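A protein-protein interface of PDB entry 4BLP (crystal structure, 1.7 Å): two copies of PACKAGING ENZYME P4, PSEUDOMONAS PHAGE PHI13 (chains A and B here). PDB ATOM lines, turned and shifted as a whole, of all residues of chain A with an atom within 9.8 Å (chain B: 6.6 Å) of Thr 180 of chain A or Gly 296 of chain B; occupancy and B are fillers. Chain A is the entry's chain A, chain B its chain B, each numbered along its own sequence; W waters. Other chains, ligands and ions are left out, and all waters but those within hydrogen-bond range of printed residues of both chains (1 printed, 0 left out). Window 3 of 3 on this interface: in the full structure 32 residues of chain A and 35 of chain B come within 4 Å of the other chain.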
ATOM      1  N   ARG A 173      -6.920  25.194  38.672  1.00  0.00           N
ATOM      2  CA  ARG A 173      -8.128  25.644  37.999  1.00  0.00           C
ATOM      3  C   ARG A 173      -9.338  25.035  38.697  1.00  0.00           C
ATOM      4  O   ARG A 173      -9.462  23.810  38.793  1.00  0.00           O
ATOM      5  CB  ARG A 173      -8.040  25.286  36.499  1.00  0.00           C
ATOM      6  CG  ARG A 173      -6.986  26.205  35.787  1.00  0.00           C
ATOM      7  CD  ARG A 173      -7.643  27.492  35.286  1.00  0.00           C
ATOM      8  NE  ARG A 173      -8.595  27.163  34.223  1.00  0.00           N
ATOM      9  CZ  ARG A 173      -9.632  27.901  33.826  1.00  0.00           C
ATOM     10  NH1 ARG A 173      -9.830  29.108  34.330  1.00  0.00           N
ATOM     11  NH2 ARG A 173     -10.433  27.462  32.875  1.00  0.00           N
ATOM     12  N   PRO A 177     -15.170  27.870  33.752  1.00  0.00           N
ATOM     13  CA  PRO A 177     -15.414  27.076  32.529  1.00  0.00           C
ATOM     14  C   PRO A 177     -14.093  26.745  31.806  1.00  0.00           C
ATOM     15  O   PRO A 177     -13.174  27.569  31.775  1.00  0.00           O
ATOM     16  CB  PRO A 177     -16.291  27.989  31.656  1.00  0.00           C
ATOM     17  CG  PRO A 177     -15.948  29.385  32.140  1.00  0.00           C
ATOM     18  CD  PRO A 177     -15.668  29.251  33.609  1.00  0.00           C
ATOM     19  N   GLY A 178     -14.034  25.551  31.240  1.00  0.00           N
ATOM     20  CA  GLY A 178     -12.881  25.053  30.491  1.00  0.00           C
ATOM     21  C   GLY A 178     -12.445  26.046  29.432  1.00  0.00           C
ATOM     22  O   GLY A 178     -13.285  26.640  28.755  1.00  0.00           O
ATOM     23  N   GLU A 179     -11.111  26.248  29.315  1.00  0.00           N
ATOM     24  CA  GLU A 179     -10.558  27.195  28.358  1.00  0.00           C
ATOM     25  C   GLU A 179      -9.246  26.632  27.798  1.00  0.00           C
ATOM     26  O   GLU A 179      -8.749  25.639  28.331  1.00  0.00           O
ATOM     27  CB  GLU A 179     -10.332  28.537  29.078  1.00  0.00           C
ATOM     28  CG  GLU A 179     -10.575  29.741  28.191  1.00  0.00           C
ATOM     29  CD  GLU A 179     -10.946  31.013  28.927  1.00  0.00           C
ATOM     30  OE1 GLU A 179     -10.727  31.092  30.158  1.00  0.00           O
ATOM     31  OE2 GLU A 179     -11.471  31.935  28.264  1.00  0.00           O
ATOM     32  N   THR A 180      -8.720  27.220  26.685  1.00  0.00           N
ATOM     33  CA  THR A 180      -7.471  26.744  26.059  1.00  0.00           C
ATOM     34  C   THR A 180      -6.361  26.615  27.111  1.00  0.00           C
ATOM     35  O   THR A 180      -5.576  25.671  27.075  1.00  0.00           O
ATOM     36  CB  THR A 180      -7.041  27.664  24.903  1.00  0.00           C
ATOM     37  OG1 THR A 180      -6.995  29.013  25.382  1.00  0.00           O
ATOM     38  CG2 THR A 180      -7.986  27.563  23.693  1.00  0.00           C
ATOM     39  N   PHE A 181      -6.339  27.524  28.075  1.00  0.00           N
ATOM     40  CA  PHE A 181      -5.360  27.513  29.180  1.00  0.00           C
ATOM     41  C   PHE A 181      -5.298  26.142  29.901  1.00  0.00           C
ATOM     42  O   PHE A 181      -4.229  25.740  30.362  1.00  0.00           O
ATOM     43  CB  PHE A 181      -5.738  28.607  30.176  1.00  0.00           C
ATOM     44  CG  PHE A 181      -4.787  28.781  31.323  1.00  0.00           C
ATOM     45  CD1 PHE A 181      -3.562  29.422  31.144  1.00  0.00           C
ATOM     46  CD2 PHE A 181      -5.117  28.322  32.592  1.00  0.00           C
ATOM     47  CE1 PHE A 181      -2.686  29.602  32.221  1.00  0.00           C
ATOM     48  CE2 PHE A 181      -4.233  28.482  33.659  1.00  0.00           C
ATOM     49  CZ  PHE A 181      -3.038  29.138  33.474  1.00  0.00           C
ATOM     50  N   ASP A 182      -6.438  25.410  29.963  1.00  0.00           N
ATOM     51  CA  ASP A 182      -6.499  24.126  30.657  1.00  0.00           C
ATOM     52  C   ASP A 182      -5.691  23.031  29.961  1.00  0.00           C
ATOM     53  O   ASP A 182      -5.341  22.052  30.616  1.00  0.00           O
ATOM     54  CB  ASP A 182      -7.956  23.696  30.858  1.00  0.00           C
ATOM     55  CG  ASP A 182      -8.645  24.617  31.845  1.00  0.00           C
ATOM     56  OD1 ASP A 182      -8.085  24.831  32.981  1.00  0.00           O
ATOM     57  OD2 ASP A 182      -9.704  25.162  31.502  1.00  0.00           O
ATOM     58  N   MET A 183      -5.312  23.232  28.708  1.00  0.00           N
ATOM     59  CA  MET A 183      -4.466  22.263  27.991  1.00  0.00           C
ATOM     60  C   MET A 183      -3.012  22.282  28.487  1.00  0.00           C
ATOM     61  O   MET A 183      -2.276  21.299  28.273  1.00  0.00           O
ATOM     62  CB  MET A 183      -4.463  22.569  26.480  1.00  0.00           C
ATOM     63  CG  MET A 183      -5.798  22.372  25.827  1.00  0.00           C
ATOM     64  SD  MET A 183      -5.804  22.774  24.061  1.00  0.00           S
ATOM     65  CE  MET A 183      -4.740  21.446  23.404  1.00  0.00           C
ATOM     66  N   GLU A 184      -2.586  23.409  29.108  1.00  0.00           N
ATOM     67  CA  GLU A 184      -1.194  23.583  29.567  1.00  0.00           C
ATOM     68  C   GLU A 184      -0.858  22.602  30.669  1.00  0.00           C
ATOM     69  O   GLU A 184      -1.692  22.343  31.547  1.00  0.00           O
ATOM     70  CB  GLU A 184      -0.940  25.013  30.048  1.00  0.00           C
ATOM     71  CG  GLU A 184      -1.098  26.064  28.964  1.00  0.00           C
ATOM     72  CD  GLU A 184      -0.717  27.491  29.308  1.00  0.00           C
ATOM     73  OE1 GLU A 184      -0.173  27.730  30.410  1.00  0.00           O
ATOM     74  OE2 GLU A 184      -0.945  28.376  28.452  1.00  0.00           O
ATOM     75  N   GLU A 185       0.374  22.060  30.621  1.00  0.00           N
ATOM     76  CA  GLU A 185       0.858  21.129  31.641  1.00  0.00           C
ATOM     77  C   GLU A 185       0.903  21.824  33.012  1.00  0.00           C
ATOM     78  O   GLU A 185       0.653  21.172  34.027  1.00  0.00           O
ATOM     79  CB  GLU A 185       2.256  20.589  31.247  1.00  0.00           C
ATOM     80  CG  GLU A 185       2.791  19.473  32.135  1.00  0.00           C
ATOM     81  CD  GLU A 185       4.195  18.987  31.813  1.00  0.00           C
ATOM     82  OE1 GLU A 185       5.030  19.798  31.351  1.00  0.00           O
ATOM     83  OE2 GLU A 185       4.470  17.790  32.055  1.00  0.00           O
ATOM     84  N   SER A 186       1.182  23.147  33.041  1.00  0.00           N
ATOM     85  CA  SER A 186       1.273  23.898  34.304  1.00  0.00           C
ATOM     86  C   SER A 186      -0.123  24.241  34.900  1.00  0.00           C
ATOM     87  O   SER A 186      -0.178  24.934  35.913  1.00  0.00           O
ATOM     88  CB  SER A 186       2.095  25.166  34.117  1.00  0.00           C
ATOM     89  OG  SER A 186       1.453  26.008  33.174  1.00  0.00           O
ATOM     90  N   SER A 187      -1.224  23.796  34.278  1.00  0.00           N
ATOM     91  CA  SER A 187      -2.549  24.038  34.861  1.00  0.00           C
ATOM     92  C   SER A 187      -3.049  22.709  35.420  1.00  0.00           C
ATOM     93  O   SER A 187      -2.998  21.700  34.720  1.00  0.00           O
ATOM     94  CB  SER A 187      -3.507  24.626  33.824  1.00  0.00           C
ATOM     95  OG  SER A 187      -3.756  23.705  32.787  1.00  0.00           O
ATOM     96  N   ALA B 131     -10.124  21.515  28.501  1.00  0.00           N
ATOM     97  CA  ALA B 131     -10.351  21.936  27.109  1.00  0.00           C
ATOM     98  C   ALA B 131      -9.296  21.317  26.272  1.00  0.00           C
ATOM     99  O   ALA B 131      -8.213  21.032  26.770  1.00  0.00           O
ATOM    100  CB  ALA B 131     -10.324  23.448  26.968  1.00  0.00           C
ATOM    101  N   SER B 132      -9.605  21.074  25.001  1.00  0.00           N
ATOM    102  CA  SER B 132      -8.649  20.472  24.071  1.00  0.00           C
ATOM    103  C   SER B 132      -8.869  21.014  22.680  1.00  0.00           C
ATOM    104  O   SER B 132     -10.013  21.185  22.248  1.00  0.00           O
ATOM    105  CB  SER B 132      -8.789  18.955  24.074  1.00  0.00           C
ATOM    106  OG  SER B 132      -7.954  18.340  23.103  1.00  0.00           O
ATOM    107  N   LEU B 133      -7.760  21.274  21.966  1.00  0.00           N
ATOM    108  CA  LEU B 133      -7.835  21.707  20.571  1.00  0.00           C
ATOM    109  C   LEU B 133      -8.356  20.559  19.696  1.00  0.00           C
ATOM    110  O   LEU B 133      -8.784  20.798  18.572  1.00  0.00           O
ATOM    111  CB  LEU B 133      -6.446  22.149  20.087  1.00  0.00           C
ATOM    112  CG  LEU B 133      -5.917  23.491  20.524  1.00  0.00           C
ATOM    113  CD1 LEU B 133      -4.494  23.704  19.997  1.00  0.00           C
ATOM    114  CD2 LEU B 133      -6.800  24.587  20.044  1.00  0.00           C
ATOM    115  N   VAL B 136     -13.137  20.254  19.351  1.00  0.00           N
ATOM    116  CA  VAL B 136     -13.773  21.517  19.010  1.00  0.00           C
ATOM    117  C   VAL B 136     -14.971  21.217  18.102  1.00  0.00           C
ATOM    118  O   VAL B 136     -15.094  20.111  17.549  1.00  0.00           O
ATOM    119  CB  VAL B 136     -12.825  22.593  18.437  1.00  0.00           C
ATOM    120  CG1 VAL B 136     -11.732  22.970  19.458  1.00  0.00           C
ATOM    121  CG2 VAL B 136     -12.211  22.149  17.113  1.00  0.00           C
ATOM    122  N   VAL B 141     -18.932  29.323  15.130  1.00  0.00           N
ATOM    123  CA  VAL B 141     -17.549  29.380  14.658  1.00  0.00           C
ATOM    124  C   VAL B 141     -17.140  27.933  14.404  1.00  0.00           C
ATOM    125  O   VAL B 141     -17.731  27.028  14.981  1.00  0.00           O
ATOM    126  CB  VAL B 141     -16.552  30.139  15.597  1.00  0.00           C
ATOM    127  CG1 VAL B 141     -16.946  31.611  15.738  1.00  0.00           C
ATOM    128  CG2 VAL B 141     -16.435  29.459  16.963  1.00  0.00           C
ATOM    129  N   ARG B 142     -16.101  27.712  13.592  1.00  0.00           N
ATOM    130  CA  ARG B 142     -15.671  26.357  13.246  1.00  0.00           C
ATOM    131  C   ARG B 142     -15.062  25.580  14.420  1.00  0.00           C
ATOM    132  O   ARG B 142     -15.014  24.352  14.380  1.00  0.00           O
ATOM    133  CB  ARG B 142     -14.650  26.409  12.085  1.00  0.00           C
ATOM    134  CG  ARG B 142     -13.406  27.252  12.422  1.00  0.00           C
ATOM    135  CD  ARG B 142     -12.120  26.839  11.711  1.00  0.00           C
ATOM    136  NE  ARG B 142     -10.946  27.486  12.317  1.00  0.00           N
ATOM    137  CZ  ARG B 142     -10.082  26.884  13.138  1.00  0.00           C
ATOM    138  NH1 ARG B 142     -10.229  25.601  13.451  1.00  0.00           N
ATOM    139  NH2 ARG B 142      -9.049  27.554  13.628  1.00  0.00           N
ATOM    140  N   ASN B 143     -14.534  26.289  15.424  1.00  0.00           N
ATOM    141  CA  ASN B 143     -13.754  25.662  16.489  1.00  0.00           C
ATOM    142  C   ASN B 143     -14.223  26.063  17.879  1.00  0.00           C
ATOM    143  O   ASN B 143     -13.405  26.411  18.726  1.00  0.00           O
ATOM    144  CB  ASN B 143     -12.283  26.051  16.311  1.00  0.00           C
ATOM    145  CG  ASN B 143     -12.014  27.532  16.344  1.00  0.00           C
ATOM    146  OD1 ASN B 143     -12.909  28.368  16.163  1.00  0.00           O
ATOM    147  ND2 ASN B 143     -10.779  27.893  16.630  1.00  0.00           N
ATOM    148  N   HIS B 144     -15.533  25.963  18.123  1.00  0.00           N
ATOM    149  CA  HIS B 144     -16.098  26.248  19.442  1.00  0.00           C
ATOM    150  C   HIS B 144     -15.576  25.194  20.435  1.00  0.00           C
ATOM    151  O   HIS B 144     -15.570  24.006  20.099  1.00  0.00           O
ATOM    152  CB  HIS B 144     -17.636  26.143  19.309  1.00  0.00           C
ATOM    153  CG  HIS B 144     -18.427  26.756  20.428  1.00  0.00           C
ATOM    154  ND1 HIS B 144     -18.265  26.344  21.744  1.00  0.00           N
ATOM    155  CD2 HIS B 144     -19.407  27.688  20.376  1.00  0.00           C
ATOM    156  CE1 HIS B 144     -19.140  27.042  22.454  1.00  0.00           C
ATOM    157  NE2 HIS B 144     -19.837  27.882  21.683  1.00  0.00           N
ATOM    158  N   LEU B 145     -15.100  25.592  21.624  1.00  0.00           N
ATOM    159  CA  LEU B 145     -14.656  24.577  22.567  1.00  0.00           C
ATOM    160  C   LEU B 145     -15.826  23.698  23.030  1.00  0.00           C
ATOM    161  O   LEU B 145     -16.999  24.133  22.983  1.00  0.00           O
ATOM    162  CB  LEU B 145     -13.987  25.233  23.811  1.00  0.00           C
ATOM    163  CG  LEU B 145     -12.603  25.873  23.587  1.00  0.00           C
ATOM    164  CD1 LEU B 145     -12.095  26.484  24.882  1.00  0.00           C
ATOM    165  CD2 LEU B 145     -11.581  24.858  23.122  1.00  0.00           C
ATOM    166  N   ARG B 294     -15.724  30.899  23.570  1.00  0.00           N
ATOM    167  CA  ARG B 294     -14.386  30.410  23.885  1.00  0.00           C
ATOM    168  C   ARG B 294     -14.072  29.426  22.785  1.00  0.00           C
ATOM    169  O   ARG B 294     -14.710  28.361  22.720  1.00  0.00           O
ATOM    170  CB  ARG B 294     -14.342  29.728  25.274  1.00  0.00           C
ATOM    171  CG  ARG B 294     -14.709  30.654  26.425  1.00  0.00           C
ATOM    172  CD  ARG B 294     -14.711  29.971  27.781  1.00  0.00           C
ATOM    173  NE  ARG B 294     -15.562  30.750  28.700  1.00  0.00           N
ATOM    174  CZ  ARG B 294     -15.152  31.769  29.447  1.00  0.00           C
ATOM    175  NH1 ARG B 294     -13.872  32.122  29.457  1.00  0.00           N
ATOM    176  NH2 ARG B 294     -16.014  32.433  30.203  1.00  0.00           N
ATOM    177  N   SER B 295     -13.157  29.802  21.867  1.00  0.00           N
ATOM    178  CA  SER B 295     -12.814  28.950  20.753  1.00  0.00           C
ATOM    179  C   SER B 295     -11.403  28.377  20.946  1.00  0.00           C
ATOM    180  O   SER B 295     -10.645  28.830  21.825  1.00  0.00           O
ATOM    181  CB  SER B 295     -12.907  29.740  19.441  1.00  0.00           C
ATOM    182  OG  SER B 295     -11.710  30.468  19.150  1.00  0.00           O
ATOM    183  N   GLY B 296     -11.049  27.400  20.114  1.00  0.00           N
ATOM    184  CA  GLY B 296      -9.706  26.811  20.137  1.00  0.00           C
ATOM    185  C   GLY B 296      -8.605  27.828  19.882  1.00  0.00           C
ATOM    186  O   GLY B 296      -7.460  27.613  20.287  1.00  0.00           O
ATOM    187  N   THR B 297      -8.941  28.970  19.260  1.00  0.00           N
ATOM    188  CA  THR B 297      -7.966  30.020  18.931  1.00  0.00           C
ATOM    189  C   THR B 297      -8.168  31.311  19.752  1.00  0.00           C
ATOM    190  O   THR B 297      -7.697  32.376  19.349  1.00  0.00           O
ATOM    191  CB  THR B 297      -7.993  30.313  17.423  1.00  0.00           C
ATOM    192  OG1 THR B 297      -9.319  30.658  17.013  1.00  0.00           O
ATOM    193  CG2 THR B 297      -7.504  29.147  16.615  1.00  0.00           C
ATOM    194  N   GLY B 298      -8.869  31.204  20.885  1.00  0.00           N
ATOM    195  CA  GLY B 298      -9.113  32.320  21.788  1.00  0.00           C
ATOM    196  C   GLY B 298     -10.563  32.759  21.889  1.00  0.00           C
ATOM    197  O   GLY B 298     -11.441  32.169  21.249  1.00  0.00           O
ATOM    198  N   ILE B 300     -13.794  34.914  21.220  1.00  0.00           N
ATOM    199  CA  ILE B 300     -14.370  35.626  20.072  1.00  0.00           C
ATOM    200  C   ILE B 300     -15.566  36.419  20.604  1.00  0.00           C
ATOM    201  O   ILE B 300     -16.355  35.871  21.386  1.00  0.00           O
ATOM    202  CB  ILE B 300     -14.754  34.643  18.924  1.00  0.00           C
ATOM    203  CG1 ILE B 300     -13.510  33.878  18.422  1.00  0.00           C
ATOM    204  CG2 ILE B 300     -15.485  35.351  17.757  1.00  0.00           C
ATOM    205  CD1 ILE B 300     -13.848  32.692  17.575  1.00  0.00           C
HETATM  206  O   HOH W   1      -7.535  20.169  29.874  1.00  0.00           O
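OE2 of Glu 179 of chain A lies within salt-bridge range of NH1 of Arg 294 of chain B (2.7 Å). SD of Met 183 of chain A is in hydrogen-bond range of N of Leu 133 of chain B, 3.2 Å away.
The backbone NH (N) of Glu 179 of chain A is in hydrogen-bond range of the side-chain carboxylate (OD2) of Asp 182 of chain A (2.8 Å). N of Leu 145 of chain B lies within hydrogen-bond range of O of Arg 294 of chain B. NH2 of Arg 173 of chain A is in hydrogen-bond range of O of Pro 177 of chain A, 3.0 Å away. N of Thr 297 of chain B lies close to OG of Ser 295 of chain B (3.2 Å). NE of Arg 173 of chain A is in salt-bridge range of OD1 of Asp 182 of chain A (2.7 Å). N of Gly 296 of chain B sits at hydrogen-bond distance from O of Asn 143 of chain B.
Among the printed residues, pairs that only touch across the chains: Met 183 of chain A with Ala 131 of chain B, Glu 179 of chain A with Ala 131 of chain B, Thr 180 of chain A with Gly 296 of chain B, Thr 180 of chain A with Ser 295 of chain B, Pro 177 of chain A with Arg 294 of chain B, Met 183 of chain A with Ser 132 of chain B, Gly 178 of chain A with Arg 294 of chain B, Glu 179 of chain A with Leu 145 of chain B, Asp 182 of chain A with Ala 131 of chain B and Thr 180 of chain A with Leu 145 of chain B.
Printed residues of chain B within 4 Å of Thr 180 of chain A: Leu 145 (3.9 Å), Ser 295 (3.5 Å) and Gly 296 (3.4 Å). Of the printed residues of chain A, Gly 296 of chain B touches Thr 180. No residue of chain A comes within 4 Å of Gly 298 of chain B. Of the printed residues of chain B, Met 183 of chain A touches Ala 131 (2.9 Å), Ser 132 (3.7 Å) and Leu 133 (3.2 Å). Of the printed residues of chain B, Asp 182 of chain A touches Ala 131. The nearest printed residue of chain B that does not touch Thr 180 of chain A is Ala 131 of chain B (4.1 Å). The nearest printed residue of chain A that does not touch Gly 296 of chain B is Met 183 of chain A (6.4 Å). The nearest printed residue of chain B that does not touch Asp 182 of chain A is Ser 132 of chain B (6.6 Å).
Hydrophobic or aromatic side chains of chain A that line the printed part of chain B: Pro 177 and Met 183. Printed residues of chain B that touch a printed residue of chain A: Ala 131, Ser 132, Leu 133, Leu 145, Arg 294, Ser 295 and Gly 296. Along chain B the printed residues that touch a printed residue of chain A span positions 131 to 296.
No position is printed for both chains. Of the 12 pairs that touch across the chains among the printed residues, none has its exchanged pair printed and touching as well.
Water W1 bridges the backbone carbonyl oxygen (O) of Asp 182 of chain A (3.0 Å) and the backbone NH (N) of Ala 131 of chain B (3.2 Å).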
